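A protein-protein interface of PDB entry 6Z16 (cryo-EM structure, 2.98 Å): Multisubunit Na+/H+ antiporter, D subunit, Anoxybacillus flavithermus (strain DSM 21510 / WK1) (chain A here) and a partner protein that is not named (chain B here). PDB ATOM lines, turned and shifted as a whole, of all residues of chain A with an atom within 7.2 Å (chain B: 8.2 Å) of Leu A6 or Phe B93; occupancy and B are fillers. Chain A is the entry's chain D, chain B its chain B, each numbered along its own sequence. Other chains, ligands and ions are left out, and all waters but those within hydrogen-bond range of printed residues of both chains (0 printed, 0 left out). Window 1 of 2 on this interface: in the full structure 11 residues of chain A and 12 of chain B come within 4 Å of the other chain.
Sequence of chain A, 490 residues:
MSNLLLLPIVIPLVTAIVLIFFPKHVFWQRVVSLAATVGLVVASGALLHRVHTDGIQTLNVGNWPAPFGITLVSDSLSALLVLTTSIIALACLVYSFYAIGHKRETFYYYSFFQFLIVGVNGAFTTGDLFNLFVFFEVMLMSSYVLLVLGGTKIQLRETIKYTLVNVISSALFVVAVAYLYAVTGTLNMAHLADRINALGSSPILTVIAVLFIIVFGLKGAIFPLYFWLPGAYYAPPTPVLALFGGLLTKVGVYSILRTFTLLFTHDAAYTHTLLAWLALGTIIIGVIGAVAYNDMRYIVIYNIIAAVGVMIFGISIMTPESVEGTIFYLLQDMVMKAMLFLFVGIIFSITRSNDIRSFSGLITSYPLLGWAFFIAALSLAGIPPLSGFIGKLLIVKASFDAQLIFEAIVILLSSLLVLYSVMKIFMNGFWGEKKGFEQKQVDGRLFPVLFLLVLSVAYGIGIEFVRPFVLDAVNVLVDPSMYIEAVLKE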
ATOM      1  N   SER A   2      18.790 -10.801  15.023  1.00  0.00           N
ATOM      2  CA  SER A   2      19.633 -11.028  16.189  1.00  0.00           C
ATOM      3  C   SER A   2      19.860  -9.775  17.020  1.00  0.00           C
ATOM      4  O   SER A   2      20.523  -9.858  18.057  1.00  0.00           O
ATOM      5  CB  SER A   2      20.982 -11.612  15.763  1.00  0.00           C
ATOM      6  OG  SER A   2      20.826 -12.909  15.216  1.00  0.00           O
ATOM      7  N   ASN A   3      19.337  -8.628  16.601  1.00  0.00           N
ATOM      8  CA  ASN A   3      19.418  -7.398  17.375  1.00  0.00           C
ATOM      9  C   ASN A   3      18.279  -7.251  18.368  1.00  0.00           C
ATOM     10  O   ASN A   3      18.155  -6.187  18.986  1.00  0.00           O
ATOM     11  CB  ASN A   3      19.442  -6.186  16.446  1.00  0.00           C
ATOM     12  CG  ASN A   3      20.775  -6.000  15.775  1.00  0.00           C
ATOM     13  OD1 ASN A   3      21.815  -6.083  16.415  1.00  0.00           O
ATOM     14  ND2 ASN A   3      20.755  -5.759  14.475  1.00  0.00           N
ATOM     15  N   LEU A   4      17.456  -8.297  18.531  1.00  0.00           N
ATOM     16  CA  LEU A   4      16.354  -8.293  19.492  1.00  0.00           C
ATOM     17  C   LEU A   4      16.846  -8.054  20.910  1.00  0.00           C
ATOM     18  O   LEU A   4      16.175  -7.378  21.701  1.00  0.00           O
ATOM     19  CB  LEU A   4      15.612  -9.626  19.409  1.00  0.00           C
ATOM     20  CG  LEU A   4      14.424  -9.926  20.321  1.00  0.00           C
ATOM     21  CD1 LEU A   4      13.262  -9.005  20.056  1.00  0.00           C
ATOM     22  CD2 LEU A   4      14.010 -11.362  20.128  1.00  0.00           C
ATOM     23  N   LEU A   5      18.048  -8.549  21.206  1.00  0.00           N
ATOM     24  CA  LEU A   5      18.697  -8.356  22.493  1.00  0.00           C
ATOM     25  C   LEU A   5      18.935  -6.881  22.801  1.00  0.00           C
ATOM     26  O   LEU A   5      18.951  -6.493  23.973  1.00  0.00           O
ATOM     27  CB  LEU A   5      20.013  -9.130  22.479  1.00  0.00           C
ATOM     28  CG  LEU A   5      20.743  -9.580  23.731  1.00  0.00           C
ATOM     29  CD1 LEU A   5      21.595 -10.758  23.337  1.00  0.00           C
ATOM     30  CD2 LEU A   5      21.588  -8.500  24.329  1.00  0.00           C
ATOM     31  N   LEU A   6      19.117  -6.045  21.778  1.00  0.00           N
ATOM     32  CA  LEU A   6      19.291  -4.622  22.035  1.00  0.00           C
ATOM     33  C   LEU A   6      17.989  -3.868  22.185  1.00  0.00           C
ATOM     34  O   LEU A   6      18.030  -2.699  22.575  1.00  0.00           O
ATOM     35  CB  LEU A   6      20.084  -3.937  20.934  1.00  0.00           C
ATOM     36  CG  LEU A   6      21.588  -3.907  21.122  1.00  0.00           C
ATOM     37  CD1 LEU A   6      22.211  -5.186  20.676  1.00  0.00           C
ATOM     38  CD2 LEU A   6      22.156  -2.732  20.399  1.00  0.00           C
ATOM     39  N   LEU A   7      16.855  -4.482  21.863  1.00  0.00           N
ATOM     40  CA  LEU A   7      15.591  -3.767  21.986  1.00  0.00           C
ATOM     41  C   LEU A   7      15.198  -3.360  23.411  1.00  0.00           C
ATOM     42  O   LEU A   7      14.498  -2.344  23.537  1.00  0.00           O
ATOM     43  CB  LEU A   7      14.479  -4.582  21.314  1.00  0.00           C
ATOM     44  CG  LEU A   7      14.641  -4.569  19.793  1.00  0.00           C
ATOM     45  CD1 LEU A   7      13.623  -5.444  19.112  1.00  0.00           C
ATOM     46  CD2 LEU A   7      14.524  -3.155  19.278  1.00  0.00           C
ATOM     47  N   PRO A   8      15.588  -4.044  24.496  1.00  0.00           N
ATOM     48  CA  PRO A   8      15.466  -3.394  25.810  1.00  0.00           C
ATOM     49  C   PRO A   8      16.380  -2.196  26.027  1.00  0.00           C
ATOM     50  O   PRO A   8      16.092  -1.386  26.915  1.00  0.00           O
ATOM     51  CB  PRO A   8      15.793  -4.521  26.790  1.00  0.00           C
ATOM     52  CG  PRO A   8      16.422  -5.583  25.996  1.00  0.00           C
ATOM     53  CD  PRO A   8      15.757  -5.498  24.676  1.00  0.00           C
ATOM     54  N   ILE A   9      17.455  -2.045  25.262  1.00  0.00           N
ATOM     55  CA  ILE A   9      18.384  -0.938  25.445  1.00  0.00           C
ATOM     56  C   ILE A   9      18.100   0.203  24.476  1.00  0.00           C
ATOM     57  O   ILE A   9      18.075   1.368  24.876  1.00  0.00           O
ATOM     58  CB  ILE A   9      19.835  -1.445  25.299  1.00  0.00           C
ATOM     59  CG1 ILE A   9      20.110  -2.563  26.301  1.00  0.00           C
ATOM     60  CG2 ILE A   9      20.817  -0.326  25.531  1.00  0.00           C
ATOM     61  CD1 ILE A   9      21.405  -3.296  26.058  1.00  0.00           C
ATOM     62  N   VAL A  10      17.847  -0.127  23.208  1.00  0.00           N
ATOM     63  CA  VAL A  10      17.715   0.877  22.153  1.00  0.00           C
ATOM     64  C   VAL A  10      16.389   1.625  22.263  1.00  0.00           C
ATOM     65  O   VAL A  10      16.341   2.847  22.080  1.00  0.00           O
ATOM     66  CB  VAL A  10      17.891   0.195  20.782  1.00  0.00           C
ATOM     67  CG1 VAL A  10      17.571   1.133  19.643  1.00  0.00           C
ATOM     68  CG2 VAL A  10      19.309  -0.301  20.634  1.00  0.00           C
ATOM     69  N   ILE A  11      15.303   0.911  22.591  1.00  0.00           N
ATOM     70  CA  ILE A  11      13.968   1.528  22.604  1.00  0.00           C
ATOM     71  C   ILE A  11      13.804   2.653  23.629  1.00  0.00           C
ATOM     72  O   ILE A  11      13.267   3.711  23.260  1.00  0.00           O
ATOM     73  CB  ILE A  11      12.885   0.439  22.728  1.00  0.00           C
ATOM     74  CG1 ILE A  11      12.826  -0.405  21.458  1.00  0.00           C
ATOM     75  CG2 ILE A  11      11.514   1.023  23.028  1.00  0.00           C
ATOM     76  CD1 ILE A  11      11.930  -1.606  21.578  1.00  0.00           C
ATOM     77  N   PRO A  12      14.244   2.525  24.897  1.00  0.00           N
ATOM     78  CA  PRO A  12      14.120   3.698  25.778  1.00  0.00           C
ATOM     79  C   PRO A  12      15.074   4.815  25.408  1.00  0.00           C
ATOM     80  O   PRO A  12      14.687   5.989  25.495  1.00  0.00           O
ATOM     81  CB  PRO A  12      14.430   3.135  27.169  1.00  0.00           C
ATOM     82  CG  PRO A  12      14.252   1.710  27.059  1.00  0.00           C
ATOM     83  CD  PRO A  12      14.696   1.368  25.696  1.00  0.00           C
ATOM     84  N   LEU A  13      16.274   4.455  24.936  1.00  0.00           N
ATOM     85  CA  LEU A  13      17.327   5.406  24.591  1.00  0.00           C
ATOM     86  C   LEU A  13      16.857   6.416  23.557  1.00  0.00           C
ATOM     87  O   LEU A  13      16.828   7.625  23.830  1.00  0.00           O
ATOM     88  CB  LEU A  13      18.546   4.641  24.080  1.00  0.00           C
ATOM     89  CG  LEU A  13      19.743   5.499  23.701  1.00  0.00           C
ATOM     90  CD1 LEU A  13      20.185   6.274  24.908  1.00  0.00           C
ATOM     91  CD2 LEU A  13      20.859   4.631  23.185  1.00  0.00           C
ATOM     92  N   LEU A  47      11.873 -11.182  23.877  1.00  0.00           N
ATOM     93  CA  LEU A  47      13.233 -11.626  24.183  1.00  0.00           C
ATOM     94  C   LEU A  47      13.233 -12.811  25.139  1.00  0.00           C
ATOM     95  O   LEU A  47      14.047 -13.732  24.992  1.00  0.00           O
ATOM     96  CB  LEU A  47      14.047 -10.471  24.764  1.00  0.00           C
ATOM     97  CG  LEU A  47      15.487 -10.805  25.155  1.00  0.00           C
ATOM     98  CD1 LEU A  47      16.270 -11.283  23.952  1.00  0.00           C
ATOM     99  CD2 LEU A  47      16.156  -9.621  25.801  1.00  0.00           C
ATOM    100  N   LEU A  59      25.451 -11.511  21.294  1.00  0.00           N
ATOM    101  CA  LEU A  59      25.617 -10.624  20.152  1.00  0.00           C
ATOM    102  C   LEU A  59      26.876  -9.794  20.315  1.00  0.00           C
ATOM    103  O   LEU A  59      27.000  -9.029  21.273  1.00  0.00           O
ATOM    104  CB  LEU A  59      24.418  -9.698  19.972  1.00  0.00           C
ATOM    105  CG  LEU A  59      24.615  -8.818  18.741  1.00  0.00           C
ATOM    106  CD1 LEU A  59      24.730  -9.647  17.472  1.00  0.00           C
ATOM    107  CD2 LEU A  59      23.478  -7.898  18.615  1.00  0.00           C
ATOM    108  N   ASN A  60      27.797  -9.943  19.371  1.00  0.00           N
ATOM    109  CA  ASN A  60      28.922  -9.032  19.268  1.00  0.00           C
ATOM    110  C   ASN A  60      28.425  -7.717  18.689  1.00  0.00           C
ATOM    111  O   ASN A  60      27.641  -7.715  17.739  1.00  0.00           O
ATOM    112  CB  ASN A  60      29.985  -9.633  18.363  1.00  0.00           C
ATOM    113  CG  ASN A  60      30.418 -10.999  18.812  1.00  0.00           C
ATOM    114  OD1 ASN A  60      30.555 -11.259  19.996  1.00  0.00           O
ATOM    115  ND2 ASN A  60      30.632 -11.886  17.861  1.00  0.00           N
ATOM    116  N   VAL A  61      28.860  -6.596  19.271  1.00  0.00           N
ATOM    117  CA  VAL A  61      28.353  -5.296  18.837  1.00  0.00           C
ATOM    118  C   VAL A  61      28.827  -4.987  17.424  1.00  0.00           C
ATOM    119  O   VAL A  61      28.031  -4.982  16.484  1.00  0.00           O
ATOM    120  CB  VAL A  61      28.741  -4.192  19.833  1.00  0.00           C
ATOM    121  CG1 VAL A  61      28.371  -2.842  19.286  1.00  0.00           C
ATOM    122  CG2 VAL A  61      28.005  -4.406  21.131  1.00  0.00           C
ATOM    123  N   GLY A  62      30.130  -4.868  17.217  1.00  0.00           N
ATOM    124  CA  GLY A  62      30.616  -4.878  15.854  1.00  0.00           C
ATOM    125  C   GLY A  62      30.557  -6.283  15.269  1.00  0.00           C
ATOM    126  O   GLY A  62      29.958  -7.208  15.816  1.00  0.00           O
ATOM    127  N   ASN A  63      31.231  -6.456  14.145  1.00  0.00           N
ATOM    128  CA  ASN A  63      31.418  -7.811  13.659  1.00  0.00           C
ATOM    129  C   ASN A  63      32.691  -8.439  14.241  1.00  0.00           C
ATOM    130  O   ASN A  63      33.241  -9.381  13.660  1.00  0.00           O
ATOM    131  CB  ASN A  63      31.428  -7.824  12.129  1.00  0.00           C
ATOM    132  CG  ASN A  63      31.034  -9.171  11.551  1.00  0.00           C
ATOM    133  OD1 ASN A  63      30.695 -10.093  12.285  1.00  0.00           O
ATOM    134  ND2 ASN A  63      31.091  -9.292  10.232  1.00  0.00           N
ATOM    135  N   LEU A  72      27.298  -8.524  24.111  1.00  0.00           N
ATOM    136  CA  LEU A  72      26.113  -8.469  24.947  1.00  0.00           C
ATOM    137  C   LEU A  72      25.515  -9.862  25.040  1.00  0.00           C
ATOM    138  O   LEU A  72      25.305 -10.521  24.019  1.00  0.00           O
ATOM    139  CB  LEU A  72      25.096  -7.491  24.377  1.00  0.00           C
ATOM    140  CG  LEU A  72      25.481  -6.025  24.372  1.00  0.00           C
ATOM    141  CD1 LEU A  72      24.392  -5.246  23.695  1.00  0.00           C
ATOM    142  CD2 LEU A  72      25.686  -5.534  25.778  1.00  0.00           C
ATOM    143  N   THR A 125      22.015  -6.707  30.985  1.00  0.00           N
ATOM    144  CA  THR A 125      22.595  -7.432  29.855  1.00  0.00           C
ATOM    145  C   THR A 125      23.866  -6.732  29.374  1.00  0.00           C
ATOM    146  O   THR A 125      23.824  -5.736  28.647  1.00  0.00           O
ATOM    147  CB  THR A 125      21.572  -7.657  28.727  1.00  0.00           C
ATOM    148  OG1 THR A 125      22.225  -8.231  27.588  1.00  0.00           O
ATOM    149  CG2 THR A 125      20.753  -6.412  28.341  1.00  0.00           C
ATOM    150  N   ALA B  79      24.589   9.394  16.401  1.00  0.00           N
ATOM    151  CA  ALA B  79      25.254   8.164  16.839  1.00  0.00           C
ATOM    152  C   ALA B  79      24.306   6.960  16.798  1.00  0.00           C
ATOM    153  O   ALA B  79      24.652   5.886  16.264  1.00  0.00           O
ATOM    154  CB  ALA B  79      25.827   8.362  18.239  1.00  0.00           C
ATOM    155  N   VAL B  80      23.078   7.142  17.303  1.00  0.00           N
ATOM    156  CA  VAL B  80      22.110   6.048  17.322  1.00  0.00           C
ATOM    157  C   VAL B  80      21.678   5.680  15.903  1.00  0.00           C
ATOM    158  O   VAL B  80      21.525   4.497  15.578  1.00  0.00           O
ATOM    159  CB  VAL B  80      20.915   6.419  18.219  1.00  0.00           C
ATOM    160  CG1 VAL B  80      19.858   5.342  18.190  1.00  0.00           C
ATOM    161  CG2 VAL B  80      21.375   6.620  19.644  1.00  0.00           C
ATOM    162  N   GLY B  81      21.537   6.672  15.021  1.00  0.00           N
ATOM    163  CA  GLY B  81      21.152   6.399  13.650  1.00  0.00           C
ATOM    164  C   GLY B  81      22.236   5.721  12.843  1.00  0.00           C
ATOM    165  O   GLY B  81      21.930   4.934  11.941  1.00  0.00           O
ATOM    166  N   THR B  82      23.506   6.012  13.148  1.00  0.00           N
ATOM    167  CA  THR B  82      24.604   5.232  12.586  1.00  0.00           C
ATOM    168  C   THR B  82      24.486   3.768  12.983  1.00  0.00           C
ATOM    169  O   THR B  82      24.622   2.867  12.138  1.00  0.00           O
ATOM    170  CB  THR B  82      25.938   5.806  13.057  1.00  0.00           C
ATOM    171  OG1 THR B  82      26.033   7.178  12.659  1.00  0.00           O
ATOM    172  CG2 THR B  82      27.087   5.036  12.454  1.00  0.00           C
ATOM    173  N   GLY B  83      24.158   3.517  14.254  1.00  0.00           N
ATOM    174  CA  GLY B  83      23.917   2.142  14.680  1.00  0.00           C
ATOM    175  C   GLY B  83      22.716   1.485  14.014  1.00  0.00           C
ATOM    176  O   GLY B  83      22.759   0.304  13.659  1.00  0.00           O
ATOM    177  N   MET B  84      21.634   2.242  13.816  1.00  0.00           N
ATOM    178  CA  MET B  84      20.427   1.658  13.228  1.00  0.00           C
ATOM    179  C   MET B  84      20.629   1.333  11.752  1.00  0.00           C
ATOM    180  O   MET B  84      20.210   0.263  11.279  1.00  0.00           O
ATOM    181  CB  MET B  84      19.232   2.593  13.407  1.00  0.00           C
ATOM    182  CG  MET B  84      18.804   2.807  14.847  1.00  0.00           C
ATOM    183  SD  MET B  84      17.225   3.669  15.001  1.00  0.00           S
ATOM    184  CE  MET B  84      17.677   5.334  14.525  1.00  0.00           C
ATOM    185  N   SER B  85      21.291   2.237  11.019  1.00  0.00           N
ATOM    186  CA  SER B  85      21.643   1.970   9.631  1.00  0.00           C
ATOM    187  C   SER B  85      22.593   0.789   9.518  1.00  0.00           C
ATOM    188  O   SER B  85      22.585   0.077   8.507  1.00  0.00           O
ATOM    189  CB  SER B  85      22.278   3.209   9.007  1.00  0.00           C
ATOM    190  OG  SER B  85      23.540   3.468   9.593  1.00  0.00           O
ATOM    191  N   SER B  86      23.412   0.557  10.546  1.00  0.00           N
ATOM    192  CA  SER B  86      24.140  -0.703  10.604  1.00  0.00           C
ATOM    193  C   SER B  86      23.214  -1.892  10.843  1.00  0.00           C
ATOM    194  O   SER B  86      23.493  -2.992  10.352  1.00  0.00           O
ATOM    195  CB  SER B  86      25.204  -0.630  11.690  1.00  0.00           C
ATOM    196  OG  SER B  86      26.163   0.373  11.401  1.00  0.00           O
ATOM    197  N   MET B  87      22.121  -1.700  11.594  1.00  0.00           N
ATOM    198  CA  MET B  87      21.264  -2.836  11.955  1.00  0.00           C
ATOM    199  C   MET B  87      20.449  -3.355  10.779  1.00  0.00           C
ATOM    200  O   MET B  87      20.194  -4.563  10.700  1.00  0.00           O
ATOM    201  CB  MET B  87      20.294  -2.490  13.082  1.00  0.00           C
ATOM    202  CG  MET B  87      20.890  -2.372  14.447  1.00  0.00           C
ATOM    203  SD  MET B  87      19.605  -2.413  15.715  1.00  0.00           S
ATOM    204  CE  MET B  87      18.810  -0.839  15.475  1.00  0.00           C
ATOM    205  N   PHE B  88      19.987  -2.466   9.889  1.00  0.00           N
ATOM    206  CA  PHE B  88      19.014  -2.907   8.883  1.00  0.00           C
ATOM    207  C   PHE B  88      19.605  -3.863   7.846  1.00  0.00           C
ATOM    208  O   PHE B  88      18.896  -4.748   7.358  1.00  0.00           O
ATOM    209  CB  PHE B  88      18.374  -1.718   8.162  1.00  0.00           C
ATOM    210  CG  PHE B  88      17.439  -0.923   9.017  1.00  0.00           C
ATOM    211  CD1 PHE B  88      16.230  -1.457   9.421  1.00  0.00           C
ATOM    212  CD2 PHE B  88      17.735   0.380   9.361  1.00  0.00           C
ATOM    213  CE1 PHE B  88      15.358  -0.720  10.204  1.00  0.00           C
ATOM    214  CE2 PHE B  88      16.870   1.122  10.141  1.00  0.00           C
ATOM    215  CZ  PHE B  88      15.680   0.572  10.559  1.00  0.00           C
ATOM    216  N   ASP B  90      21.358  -6.620   7.578  1.00  0.00           N
ATOM    217  CA  ASP B  90      21.781  -7.965   8.020  1.00  0.00           C
ATOM    218  C   ASP B  90      23.103  -7.957   8.792  1.00  0.00           C
ATOM    219  O   ASP B  90      23.918  -8.873   8.670  1.00  0.00           O
ATOM    220  CB  ASP B  90      21.864  -8.946   6.845  1.00  0.00           C
ATOM    221  CG  ASP B  90      20.504  -9.405   6.373  1.00  0.00           C
ATOM    222  OD1 ASP B  90      19.585  -9.482   7.214  1.00  0.00           O
ATOM    223  OD2 ASP B  90      20.354  -9.691   5.166  1.00  0.00           O
ATOM    224  N   ARG B  91      23.321  -6.923   9.590  1.00  0.00           N
ATOM    225  CA  ARG B  91      24.537  -6.756  10.368  1.00  0.00           C
ATOM    226  C   ARG B  91      24.175  -6.377  11.794  1.00  0.00           C
ATOM    227  O   ARG B  91      23.081  -5.864  12.046  1.00  0.00           O
ATOM    228  CB  ARG B  91      25.448  -5.680   9.754  1.00  0.00           C
ATOM    229  CG  ARG B  91      26.024  -6.054   8.411  1.00  0.00           C
ATOM    230  CD  ARG B  91      26.949  -7.245   8.539  1.00  0.00           C
ATOM    231  NE  ARG B  91      27.569  -7.582   7.265  1.00  0.00           N
ATOM    232  CZ  ARG B  91      27.027  -8.404   6.374  1.00  0.00           C
ATOM    233  NH1 ARG B  91      25.852  -8.964   6.616  1.00  0.00           N
ATOM    234  NH2 ARG B  91      27.657  -8.658   5.236  1.00  0.00           N
ATOM    235  N   PRO B  92      25.061  -6.633  12.752  1.00  0.00           N
ATOM    236  CA  PRO B  92      24.819  -6.169  14.121  1.00  0.00           C
ATOM    237  C   PRO B  92      24.923  -4.655  14.239  1.00  0.00           C
ATOM    238  O   PRO B  92      25.321  -3.943  13.318  1.00  0.00           O
ATOM    239  CB  PRO B  92      25.916  -6.864  14.925  1.00  0.00           C
ATOM    240  CG  PRO B  92      26.288  -8.037  14.125  1.00  0.00           C
ATOM    241  CD  PRO B  92      26.154  -7.619  12.707  1.00  0.00           C
ATOM    242  N   PHE B  93      24.555  -4.178  15.421  1.00  0.00           N
ATOM    243  CA  PHE B  93      24.461  -2.753  15.718  1.00  0.00           C
ATOM    244  C   PHE B  93      25.844  -2.116  15.738  1.00  0.00           C
ATOM    245  O   PHE B  93      26.721  -2.589  16.456  1.00  0.00           O
ATOM    246  CB  PHE B  93      23.779  -2.606  17.075  1.00  0.00           C
ATOM    247  CG  PHE B  93      23.529  -1.202  17.512  1.00  0.00           C
ATOM    248  CD1 PHE B  93      22.458  -0.489  17.021  1.00  0.00           C
ATOM    249  CD2 PHE B  93      24.336  -0.615  18.463  1.00  0.00           C
ATOM    250  CE1 PHE B  93      22.207   0.791  17.452  1.00  0.00           C
ATOM    251  CE2 PHE B  93      24.096   0.669  18.892  1.00  0.00           C
ATOM    252  CZ  PHE B  93      23.033   1.375  18.384  1.00  0.00           C
ATOM    253  N   LEU B  94      26.027  -1.028  14.978  1.00  0.00           N
ATOM    254  CA  LEU B  94      27.302  -0.310  14.798  1.00  0.00           C
ATOM    255  C   LEU B  94      28.378  -1.217  14.189  1.00  0.00           C
ATOM    256  O   LEU B  94      29.382  -1.546  14.815  1.00  0.00           O
ATOM    257  CB  LEU B  94      27.813   0.310  16.109  1.00  0.00           C
ATOM    258  CG  LEU B  94      27.081   1.429  16.832  1.00  0.00           C
ATOM    259  CD1 LEU B  94      27.642   1.574  18.216  1.00  0.00           C
ATOM    260  CD2 LEU B  94      27.277   2.719  16.093  1.00  0.00           C
ATOM    261  N   THR B  95      28.141  -1.608  12.936  1.00  0.00           N
ATOM    262  CA  THR B  95      29.087  -2.419  12.171  1.00  0.00           C
ATOM    263  C   THR B  95      30.097  -1.568  11.399  1.00  0.00           C
ATOM    264  O   THR B  95      31.252  -1.988  11.241  1.00  0.00           O
ATOM    265  CB  THR B  95      28.311  -3.349  11.234  1.00  0.00           C
ATOM    266  OG1 THR B  95      27.392  -4.118  12.012  1.00  0.00           O
ATOM    267  CG2 THR B  95      29.215  -4.331  10.515  1.00  0.00           C
ATOM    268  N   HIS B  96      29.696  -0.364  10.970  1.00  0.00           N
ATOM    269  CA  HIS B  96      30.578   0.681  10.430  1.00  0.00           C
ATOM    270  C   HIS B  96      31.304   0.243   9.152  1.00  0.00           C
ATOM    271  O   HIS B  96      32.512   0.015   9.132  1.00  0.00           O
ATOM    272  CB  HIS B  96      31.580   1.171  11.483  1.00  0.00           C
ATOM    273  CG  HIS B  96      30.975   2.049  12.531  1.00  0.00           C
ATOM    274  ND1 HIS B  96      31.637   2.389  13.688  1.00  0.00           N
ATOM    275  CD2 HIS B  96      29.778   2.677  12.583  1.00  0.00           C
ATOM    276  CE1 HIS B  96      30.869   3.178  14.416  1.00  0.00           C
ATOM    277  NE2 HIS B  96      29.736   3.369  13.768  1.00  0.00           N
ATOM    278  N   PHE B 117      29.819   9.059  13.724  1.00  0.00           N
ATOM    279  CA  PHE B 117      29.745   8.791  15.156  1.00  0.00           C
ATOM    280  C   PHE B 117      30.545   9.832  15.935  1.00  0.00           C
ATOM    281  O   PHE B 117      30.052  10.413  16.915  1.00  0.00           O
ATOM    282  CB  PHE B 117      30.258   7.380  15.429  1.00  0.00           C
ATOM    283  CG  PHE B 117      30.057   6.920  16.835  1.00  0.00           C
ATOM    284  CD1 PHE B 117      28.824   6.464  17.256  1.00  0.00           C
ATOM    285  CD2 PHE B 117      31.100   6.943  17.737  1.00  0.00           C
ATOM    286  CE1 PHE B 117      28.636   6.039  18.550  1.00  0.00           C
ATOM    287  CE2 PHE B 117      30.918   6.523  19.034  1.00  0.00           C
ATOM    288  CZ  PHE B 117      29.683   6.069  19.439  1.00  0.00           C
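The side-chain amide nitrogen (ND2) of Asn A3 sits close to the side-chain sulfur (SD) of Met B87, at 3.7 Å.
The backbone carbonyl oxygen (O) of Arg B91 sits at hydrogen-bond distance from the side-chain amide nitrogen (ND2) of Asn A3 (3.4 Å).
N of Phe B93 is in hydrogen-bond range of OD1 of Asn A3, at 3.5 Å.
O of Phe B93 lies close to O of Val A61.
O of Pro B92 lies within hydrogen-bond range of OG1 of Thr B95 (2.5 Å).
The backbone carbonyl oxygen (O) of Leu A59 is in hydrogen-bond range of the backbone NH (N) of Leu A72.
CA of Pro B92 touches OD1 of Asn A3, 3.8 Å away.
CG of Phe B93 touches CD2 of Leu A6, at 3.5 Å.
CD1 of Leu A59 touches CB of Pro B92 (3.95 Å).
Asn A60 touches Pro B92 (O to CB, 3.4 Å).
Val A61 touches Pro B92.
Leu B94 touches Gly A62 (O to CA, 3.7 Å).
Of the printed residues of chain B, Asn A3 touches Met B87 (3.4 Å), Arg B91 (3.4 Å), Pro B92 (3.8 Å) and Phe B93 (3.5 Å).
Leu A5 touches none of the printed residues of chain B.
Of chain B, only Phe B93 (3.5 Å) comes within 4 Å of Leu A6.
Ile A11 touches none of the printed residues of chain B.
Printed residues of chain B within 4 Å of Leu A59: Pro B92.
Of the printed residues of chain B, Val A61 touches Pro B92 and Phe B93.
Printed residues of chain A within 4 Å of Met B87: Asn A3 (3.4 Å).
Phe B93 touches just these residues of chain A: Asn A3, Leu A6 and Val A61.
The nearest residue of chain A that does not touch Phe B93 is Gly A62 (4.2 Å).
Hydrophobic or aromatic side chains of chain B within 4 Å of the printed part of chain A: Met B87, Pro B92 and Phe B93.
Among the printed residues, 10 pairs touch across the chains.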
